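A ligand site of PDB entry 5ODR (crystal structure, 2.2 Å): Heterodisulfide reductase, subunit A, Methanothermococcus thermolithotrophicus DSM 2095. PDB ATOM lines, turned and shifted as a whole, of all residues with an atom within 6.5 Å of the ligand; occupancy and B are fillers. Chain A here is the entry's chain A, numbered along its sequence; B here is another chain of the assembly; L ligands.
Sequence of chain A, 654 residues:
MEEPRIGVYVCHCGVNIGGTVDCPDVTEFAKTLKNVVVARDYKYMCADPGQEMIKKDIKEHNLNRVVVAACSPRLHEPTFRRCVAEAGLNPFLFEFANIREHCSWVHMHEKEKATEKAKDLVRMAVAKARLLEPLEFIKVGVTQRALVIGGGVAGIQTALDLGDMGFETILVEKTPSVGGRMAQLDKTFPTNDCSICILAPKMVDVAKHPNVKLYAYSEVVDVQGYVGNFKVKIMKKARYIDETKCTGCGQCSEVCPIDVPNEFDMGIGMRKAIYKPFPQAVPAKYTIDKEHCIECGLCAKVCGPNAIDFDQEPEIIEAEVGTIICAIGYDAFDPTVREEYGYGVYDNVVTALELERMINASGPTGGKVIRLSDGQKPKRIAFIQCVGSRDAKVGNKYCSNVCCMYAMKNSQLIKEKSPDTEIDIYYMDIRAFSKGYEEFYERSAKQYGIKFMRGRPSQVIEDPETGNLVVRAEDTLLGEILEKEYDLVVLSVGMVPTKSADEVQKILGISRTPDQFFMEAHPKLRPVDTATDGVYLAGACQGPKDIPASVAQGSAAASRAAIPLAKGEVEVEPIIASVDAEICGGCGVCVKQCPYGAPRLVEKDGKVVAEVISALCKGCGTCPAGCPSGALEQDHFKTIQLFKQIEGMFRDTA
FE1 of the ligand is bound by SG of Cys 399, 2.3 Å away. SG of Cys 403 binds FE4 of the ligand (2.3 Å). The backbone NH (N) of Cys 404 lies close to a sulfur (S1) of the ligand, 3.6 Å away. The side-chain sulfur of Cys 404 binds an iron atom (FE2) of the ligand (2.3 Å). The backbone NH (N) of Cys 386 sits close to a sulfur (S1) of the ligand, 3.5 Å away. The side-chain sulfur (SG) of Cys 386 binds an iron atom (FE3) of the ligand (2.3 Å). The backbone NH (N) of Ser 400 lies close to a sulfur (S2) of the ligand (3.3 Å). A sulfur (S1) of the ligand lies close to the side-chain amide nitrogen (NE2) of Gln 385 (3.4 Å). The guanidinium group (NH1) of Arg 390 lies close to a sulfur (S4) of the ligand (3.5 Å). The backbone NH (N) of Asn 401 sits close to a sulfur (S3) of the ligand.
NE2 of Gln 385 is in hydrogen-bond range of O of Cys 403, at 3.0 Å. The backbone carbonyl oxygen (O) of Asp 429 lies close to the side-chain sulfur (SG) of Cys 404 (3.2 Å). The side-chain hydroxyl (OG) of Ser 400 sits at hydrogen-bond distance from the side-chain hydroxyl (OG) of Ser 389, at 2.8 Å. The backbone carbonyl oxygen of Tyr 398 lies within hydrogen-bond range of the backbone NH of Arg 390. The guanidinium group of Arg 431 is in salt-bridge range of the side-chain carboxylate of Asp 429 (3.6 Å). The backbone carbonyl oxygen of Ile 430 of chain B lies within hydrogen-bond range of the guanidinium group of Arg 431 (2.8 Å). ND2 of Asn 401 lies within hydrogen-bond range of O of Phe 433 of chain B. N of Ile 430 of chain B lies within hydrogen-bond range of OD1 of Asp 429, at 2.9 Å.
The backbone carbonyl oxygen (O) of Asp 429 lies close to a sulfur (S4) of the ligand (3.8 Å). Merely in contact with the ligand: Ser 389 (3.4 Å) and Arg 431 (3.5 Å). 11 residues have an atom within 4 Å of the ligand: Gln 385, Cys 386, Ser 389, Arg 390, Cys 399, Ser 400, Asn 401, Cys 403, Cys 404, Asp 429 and Arg 431.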
ATOM      1  N   ILE A 384     -19.664  21.585  -7.975  1.00  0.00           N
ATOM      2  CA  ILE A 384     -18.715  22.264  -7.107  1.00  0.00           C
ATOM      3  C   ILE A 384     -19.529  22.988  -6.054  1.00  0.00           C
ATOM      4  O   ILE A 384     -20.237  23.938  -6.385  1.00  0.00           O
ATOM      5  CB  ILE A 384     -17.797  23.205  -7.911  1.00  0.00           C
ATOM      6  CG1 ILE A 384     -16.991  22.380  -8.958  1.00  0.00           C
ATOM      7  CG2 ILE A 384     -16.867  23.975  -6.966  1.00  0.00           C
ATOM      8  CD1 ILE A 384     -15.919  23.142  -9.728  1.00  0.00           C
ATOM      9  N   GLN A 385     -19.426  22.558  -4.788  1.00  0.00           N
ATOM     10  CA  GLN A 385     -20.177  23.152  -3.688  1.00  0.00           C
ATOM     11  C   GLN A 385     -19.600  24.447  -3.150  1.00  0.00           C
ATOM     12  O   GLN A 385     -18.452  24.796  -3.420  1.00  0.00           O
ATOM     13  CB  GLN A 385     -20.292  22.140  -2.525  1.00  0.00           C
ATOM     14  CG  GLN A 385     -20.984  20.810  -2.911  1.00  0.00           C
ATOM     15  CD  GLN A 385     -22.247  21.022  -3.705  1.00  0.00           C
ATOM     16  OE1 GLN A 385     -22.278  20.837  -4.917  1.00  0.00           O
ATOM     17  NE2 GLN A 385     -23.294  21.487  -3.049  1.00  0.00           N
ATOM     18  N   CYS A 386     -20.431  25.169  -2.373  1.00  0.00           N
ATOM     19  CA  CYS A 386     -20.109  26.421  -1.703  1.00  0.00           C
ATOM     20  C   CYS A 386     -19.626  27.537  -2.640  1.00  0.00           C
ATOM     21  O   CYS A 386     -18.793  28.345  -2.217  1.00  0.00           O
ATOM     22  CB  CYS A 386     -19.112  26.175  -0.573  1.00  0.00           C
ATOM     23  SG  CYS A 386     -19.552  24.793   0.505  1.00  0.00           S
ATOM     24  N   VAL A 387     -20.132  27.619  -3.879  1.00  0.00           N
ATOM     25  CA  VAL A 387     -19.709  28.670  -4.805  1.00  0.00           C
ATOM     26  C   VAL A 387     -20.436  29.967  -4.402  1.00  0.00           C
ATOM     27  O   VAL A 387     -21.645  30.083  -4.576  1.00  0.00           O
ATOM     28  CB  VAL A 387     -19.933  28.286  -6.277  1.00  0.00           C
ATOM     29  CG1 VAL A 387     -19.487  29.406  -7.211  1.00  0.00           C
ATOM     30  CG2 VAL A 387     -19.194  26.990  -6.606  1.00  0.00           C
ATOM     31  N   SER A 389     -20.351  31.094  -1.248  1.00  0.00           N
ATOM     32  CA  SER A 389     -20.759  30.919   0.150  1.00  0.00           C
ATOM     33  C   SER A 389     -19.570  30.446   0.955  1.00  0.00           C
ATOM     34  O   SER A 389     -18.626  29.893   0.373  1.00  0.00           O
ATOM     35  CB  SER A 389     -21.871  29.877   0.253  1.00  0.00           C
ATOM     36  OG  SER A 389     -22.964  30.195  -0.586  1.00  0.00           O
ATOM     37  N   ARG A 390     -19.586  30.671   2.280  1.00  0.00           N
ATOM     38  CA  ARG A 390     -18.473  30.252   3.132  1.00  0.00           C
ATOM     39  C   ARG A 390     -17.153  30.715   2.491  1.00  0.00           C
ATOM     40  O   ARG A 390     -16.155  29.992   2.529  1.00  0.00           O
ATOM     41  CB  ARG A 390     -18.472  28.723   3.272  1.00  0.00           C
ATOM     42  CG  ARG A 390     -19.829  28.107   3.642  1.00  0.00           C
ATOM     43  CD  ARG A 390     -19.728  26.592   3.822  1.00  0.00           C
ATOM     44  NE  ARG A 390     -18.767  26.222   4.857  1.00  0.00           N
ATOM     45  CZ  ARG A 390     -18.438  24.980   5.173  1.00  0.00           C
ATOM     46  NH1 ARG A 390     -18.994  23.960   4.533  1.00  0.00           N
ATOM     47  NH2 ARG A 390     -17.547  24.746   6.130  1.00  0.00           N
ATOM     48  N   TYR A 398     -21.199  33.201   4.818  1.00  0.00           N
ATOM     49  CA  TYR A 398     -22.335  32.429   5.331  1.00  0.00           C
ATOM     50  C   TYR A 398     -22.593  31.189   4.509  1.00  0.00           C
ATOM     51  O   TYR A 398     -22.099  31.060   3.376  1.00  0.00           O
ATOM     52  CB  TYR A 398     -23.595  33.300   5.354  1.00  0.00           C
ATOM     53  CG  TYR A 398     -23.938  33.919   4.017  1.00  0.00           C
ATOM     54  CD1 TYR A 398     -23.381  35.137   3.639  1.00  0.00           C
ATOM     55  CD2 TYR A 398     -24.797  33.297   3.138  1.00  0.00           C
ATOM     56  CE1 TYR A 398     -23.675  35.718   2.409  1.00  0.00           C
ATOM     57  CE2 TYR A 398     -25.103  33.861   1.894  1.00  0.00           C
ATOM     58  CZ  TYR A 398     -24.544  35.076   1.541  1.00  0.00           C
ATOM     59  OH  TYR A 398     -24.828  35.649   0.326  1.00  0.00           O
ATOM     60  N   CYS A 399     -23.376  30.273   5.071  1.00  0.00           N
ATOM     61  CA  CYS A 399     -23.781  29.032   4.417  1.00  0.00           C
ATOM     62  C   CYS A 399     -25.093  29.372   3.675  1.00  0.00           C
ATOM     63  O   CYS A 399     -26.003  29.918   4.295  1.00  0.00           O
ATOM     64  CB  CYS A 399     -23.989  27.923   5.448  1.00  0.00           C
ATOM     65  SG  CYS A 399     -24.627  26.367   4.777  1.00  0.00           S
ATOM     66  N   SER A 400     -25.189  29.045   2.368  1.00  0.00           N
ATOM     67  CA  SER A 400     -26.410  29.335   1.612  1.00  0.00           C
ATOM     68  C   SER A 400     -27.541  28.317   1.894  1.00  0.00           C
ATOM     69  O   SER A 400     -28.613  28.403   1.284  1.00  0.00           O
ATOM     70  CB  SER A 400     -26.119  29.504   0.123  1.00  0.00           C
ATOM     71  OG  SER A 400     -25.613  30.807  -0.102  1.00  0.00           O
ATOM     72  N   ASN A 401     -27.298  27.358   2.824  1.00  0.00           N
ATOM     73  CA  ASN A 401     -28.260  26.387   3.316  1.00  0.00           C
ATOM     74  C   ASN A 401     -28.870  25.315   2.375  1.00  0.00           C
ATOM     75  O   ASN A 401     -29.090  24.193   2.834  1.00  0.00           O
ATOM     76  CB  ASN A 401     -29.415  27.193   3.922  1.00  0.00           C
ATOM     77  CG  ASN A 401     -30.495  26.400   4.573  1.00  0.00           C
ATOM     78  OD1 ASN A 401     -31.441  25.950   3.908  1.00  0.00           O
ATOM     79  ND2 ASN A 401     -30.419  26.249   5.886  1.00  0.00           N
ATOM     80  N   VAL A 402     -29.161  25.629   1.110  1.00  0.00           N
ATOM     81  CA  VAL A 402     -29.799  24.668   0.195  1.00  0.00           C
ATOM     82  C   VAL A 402     -28.914  24.022  -0.885  1.00  0.00           C
ATOM     83  O   VAL A 402     -29.413  23.148  -1.586  1.00  0.00           O
ATOM     84  CB  VAL A 402     -30.969  25.397  -0.517  1.00  0.00           C
ATOM     85  CG1 VAL A 402     -31.848  26.139   0.473  1.00  0.00           C
ATOM     86  CG2 VAL A 402     -30.447  26.351  -1.584  1.00  0.00           C
ATOM     87  N   CYS A 403     -27.667  24.451  -1.051  1.00  0.00           N
ATOM     88  CA  CYS A 403     -26.791  23.936  -2.095  1.00  0.00           C
ATOM     89  C   CYS A 403     -26.368  22.491  -1.960  1.00  0.00           C
ATOM     90  O   CYS A 403     -26.238  21.828  -2.977  1.00  0.00           O
ATOM     91  CB  CYS A 403     -25.585  24.851  -2.257  1.00  0.00           C
ATOM     92  SG  CYS A 403     -25.694  26.378  -1.301  1.00  0.00           S
ATOM     93  N   CYS A 404     -26.158  21.991  -0.746  1.00  0.00           N
ATOM     94  CA  CYS A 404     -25.765  20.587  -0.607  1.00  0.00           C
ATOM     95  C   CYS A 404     -26.914  19.727  -1.103  1.00  0.00           C
ATOM     96  O   CYS A 404     -26.717  18.808  -1.897  1.00  0.00           O
ATOM     97  CB  CYS A 404     -25.414  20.235   0.838  1.00  0.00           C
ATOM     98  SG  CYS A 404     -23.714  20.659   1.322  1.00  0.00           S
ATOM     99  N   MET A 405     -28.131  20.037  -0.620  1.00  0.00           N
ATOM    100  CA  MET A 405     -29.334  19.299  -0.982  1.00  0.00           C
ATOM    101  C   MET A 405     -29.739  19.421  -2.441  1.00  0.00           C
ATOM    102  O   MET A 405     -30.111  18.407  -3.027  1.00  0.00           O
ATOM    103  CB  MET A 405     -30.502  19.715  -0.081  1.00  0.00           C
ATOM    104  CG  MET A 405     -30.359  19.261   1.360  1.00  0.00           C
ATOM    105  SD  MET A 405     -30.339  17.466   1.616  1.00  0.00           S
ATOM    106  CE  MET A 405     -32.028  17.030   1.118  1.00  0.00           C
ATOM    107  N   MET A 428     -17.046  20.174   1.121  1.00  0.00           N
ATOM    108  CA  MET A 428     -16.280  20.404   2.354  1.00  0.00           C
ATOM    109  C   MET A 428     -17.067  19.707   3.462  1.00  0.00           C
ATOM    110  O   MET A 428     -16.524  18.879   4.191  1.00  0.00           O
ATOM    111  CB  MET A 428     -16.157  21.905   2.653  1.00  0.00           C
ATOM    112  CG  MET A 428     -15.256  22.629   1.678  1.00  0.00           C
ATOM    113  SD  MET A 428     -14.898  24.316   2.210  1.00  0.00           S
ATOM    114  CE  MET A 428     -16.425  25.104   1.818  1.00  0.00           C
ATOM    115  N   ASP A 429     -18.366  20.053   3.576  1.00  0.00           N
ATOM    116  CA  ASP A 429     -19.299  19.447   4.529  1.00  0.00           C
ATOM    117  C   ASP A 429     -20.601  19.202   3.795  1.00  0.00           C
ATOM    118  O   ASP A 429     -21.049  20.084   3.063  1.00  0.00           O
ATOM    119  CB  ASP A 429     -19.626  20.390   5.696  1.00  0.00           C
ATOM    120  CG  ASP A 429     -18.448  20.788   6.552  1.00  0.00           C
ATOM    121  OD1 ASP A 429     -17.992  19.953   7.344  1.00  0.00           O
ATOM    122  OD2 ASP A 429     -18.034  21.963   6.480  1.00  0.00           O
ATOM    123  N   ILE A 430     -21.222  18.041   3.979  1.00  0.00           N
ATOM    124  CA  ILE A 430     -22.505  17.766   3.351  1.00  0.00           C
ATOM    125  C   ILE A 430     -23.500  18.216   4.410  1.00  0.00           C
ATOM    126  O   ILE A 430     -23.508  17.664   5.504  1.00  0.00           O
ATOM    127  CB  ILE A 430     -22.722  16.287   2.959  1.00  0.00           C
ATOM    128  CG1 ILE A 430     -21.856  15.903   1.733  1.00  0.00           C
ATOM    129  CG2 ILE A 430     -24.207  16.024   2.670  1.00  0.00           C
ATOM    130  CD1 ILE A 430     -22.189  16.681   0.377  1.00  0.00           C
ATOM    131  N   ARG A 431     -24.301  19.232   4.103  1.00  0.00           N
ATOM    132  CA  ARG A 431     -25.272  19.752   5.059  1.00  0.00           C
ATOM    133  C   ARG A 431     -26.697  19.300   4.705  1.00  0.00           C
ATOM    134  O   ARG A 431     -27.395  19.959   3.937  1.00  0.00           O
ATOM    135  CB  ARG A 431     -25.106  21.279   5.201  1.00  0.00           C
ATOM    136  CG  ARG A 431     -23.756  21.587   5.850  1.00  0.00           C
ATOM    137  CD  ARG A 431     -23.432  23.047   6.095  1.00  0.00           C
ATOM    138  NE  ARG A 431     -22.196  23.169   6.869  1.00  0.00           N
ATOM    139  CZ  ARG A 431     -21.534  24.298   7.075  1.00  0.00           C
ATOM    140  NH1 ARG A 431     -20.420  24.301   7.782  1.00  0.00           N
ATOM    141  NH2 ARG A 431     -21.981  25.441   6.551  1.00  0.00           N
ATOM    142  N   PHE A 433     -29.256  18.487   7.083  1.00  0.00           N
ATOM    143  CA  PHE A 433     -29.691  18.720   8.460  1.00  0.00           C
ATOM    144  C   PHE A 433     -31.163  18.573   8.840  1.00  0.00           C
ATOM    145  O   PHE A 433     -31.439  18.501  10.040  1.00  0.00           O
ATOM    146  CB  PHE A 433     -29.246  20.155   8.846  1.00  0.00           C
ATOM    147  CG  PHE A 433     -29.671  21.185   7.819  1.00  0.00           C
ATOM    148  CD1 PHE A 433     -30.939  21.734   7.853  1.00  0.00           C
ATOM    149  CD2 PHE A 433     -28.826  21.540   6.785  1.00  0.00           C
ATOM    150  CE1 PHE A 433     -31.339  22.646   6.882  1.00  0.00           C
ATOM    151  CE2 PHE A 433     -29.222  22.457   5.827  1.00  0.00           C
ATOM    152  CZ  PHE A 433     -30.480  23.007   5.881  1.00  0.00           C
ATOM    153  N   SER A 492     -22.447  25.008  -7.759  1.00  0.00           N
ATOM    154  CA  SER A 492     -23.556  25.095  -6.819  1.00  0.00           C
ATOM    155  C   SER A 492     -23.523  26.478  -6.160  1.00  0.00           C
ATOM    156  O   SER A 492     -23.060  26.627  -5.025  1.00  0.00           O
ATOM    157  CB  SER A 492     -23.497  23.975  -5.780  1.00  0.00           C
ATOM    158  OG  SER A 492     -23.655  22.727  -6.436  1.00  0.00           O
ATOM    159  N   VAL A 493     -24.021  27.477  -6.900  1.00  0.00           N
ATOM    160  CA  VAL A 493     -24.084  28.883  -6.482  1.00  0.00           C
ATOM    161  C   VAL A 493     -24.937  29.103  -5.244  1.00  0.00           C
ATOM    162  O   VAL A 493     -25.972  28.467  -5.078  1.00  0.00           O
ATOM    163  CB  VAL A 493     -24.536  29.812  -7.638  1.00  0.00           C
ATOM    164  CG1 VAL A 493     -23.462  29.905  -8.713  1.00  0.00           C
ATOM    165  CG2 VAL A 493     -25.877  29.370  -8.228  1.00  0.00           C
ATOM    166  N   GLY A 494     -24.493  30.034  -4.402  1.00  0.00           N
ATOM    167  CA  GLY A 494     -25.192  30.381  -3.173  1.00  0.00           C
ATOM    168  C   GLY A 494     -26.322  31.369  -3.407  1.00  0.00           C
ATOM    169  O   GLY A 494     -26.634  31.699  -4.552  1.00  0.00           O
ATOM    170  N   ILE B 430     -19.549  19.414   9.770  1.00  0.00           N
ATOM    171  CA  ILE B 430     -19.949  20.474  10.686  1.00  0.00           C
ATOM    172  C   ILE B 430     -21.177  21.060  10.011  1.00  0.00           C
ATOM    173  O   ILE B 430     -21.069  21.559   8.894  1.00  0.00           O
ATOM    174  CB  ILE B 430     -18.857  21.548  10.915  1.00  0.00           C
ATOM    175  CG1 ILE B 430     -17.703  20.990  11.786  1.00  0.00           C
ATOM    176  CG2 ILE B 430     -19.455  22.797  11.551  1.00  0.00           C
ATOM    177  CD1 ILE B 430     -18.108  20.576  13.272  1.00  0.00           C
ATOM    178  N   ALA B 432     -23.504  23.903  10.155  1.00  0.00           N
ATOM    179  CA  ALA B 432     -23.731  25.304  10.559  1.00  0.00           C
ATOM    180  C   ALA B 432     -24.359  25.941   9.328  1.00  0.00           C
ATOM    181  O   ALA B 432     -23.754  26.752   8.627  1.00  0.00           O
ATOM    182  CB  ALA B 432     -22.383  25.939  10.892  1.00  0.00           C
ATOM    183  N   PHE B 433     -25.595  25.527   9.070  1.00  0.00           N
ATOM    184  CA  PHE B 433     -26.428  25.863   7.916  1.00  0.00           C
ATOM    185  C   PHE B 433     -27.321  27.107   7.939  1.00  0.00           C
ATOM    186  O   PHE B 433     -27.795  27.495   6.867  1.00  0.00           O
ATOM    187  CB  PHE B 433     -27.333  24.650   7.633  1.00  0.00           C
ATOM    188  CG  PHE B 433     -28.065  24.177   8.873  1.00  0.00           C
ATOM    189  CD1 PHE B 433     -29.256  24.766   9.267  1.00  0.00           C
ATOM    190  CD2 PHE B 433     -27.530  23.183   9.669  1.00  0.00           C
ATOM    191  CE1 PHE B 433     -29.903  24.353  10.418  1.00  0.00           C
ATOM    192  CE2 PHE B 433     -28.178  22.778  10.826  1.00  0.00           C
ATOM    193  CZ  PHE B 433     -29.361  23.367  11.187  1.00  0.00           C
ATOM    194  N   GLU B 438     -22.459  29.632  10.215  1.00  0.00           N
ATOM    195  CA  GLU B 438     -21.134  29.403   9.637  1.00  0.00           C
ATOM    196  C   GLU B 438     -20.124  30.363  10.294  1.00  0.00           C
ATOM    197  O   GLU B 438     -18.977  29.988  10.554  1.00  0.00           O
ATOM    198  CB  GLU B 438     -21.177  29.623   8.117  1.00  0.00           C
ATOM    199  CG  GLU B 438     -19.849  29.439   7.396  1.00  0.00           C
ATOM    200  CD  GLU B 438     -19.284  28.045   7.449  1.00  0.00           C
ATOM    201  OE1 GLU B 438     -20.059  27.098   7.729  1.00  0.00           O
ATOM    202  OE2 GLU B 438     -18.075  27.879   7.186  1.00  0.00           O
HETATM  203 FE1  LIG L   1     -23.651  25.363   2.997  1.00  0.00          FE
HETATM  204 FE2  LIG L   1     -23.759  22.964   1.440  1.00  0.00          FE
HETATM  205 FE3  LIG L   1     -21.843  24.977   0.992  1.00  0.00          FE
HETATM  206 FE4  LIG L   1     -24.433  25.323   0.316  1.00  0.00          FE
HETATM  207  S1  LIG L   1     -23.008  23.768  -0.555  1.00  0.00           S
HETATM  208  S2  LIG L   1     -22.969  26.860   1.344  1.00  0.00           S
HETATM  209  S3  LIG L   1     -25.483  24.264   2.076  1.00  0.00           S
HETATM  210  S4  LIG L   1     -22.080  23.724   2.914  1.00  0.00           S
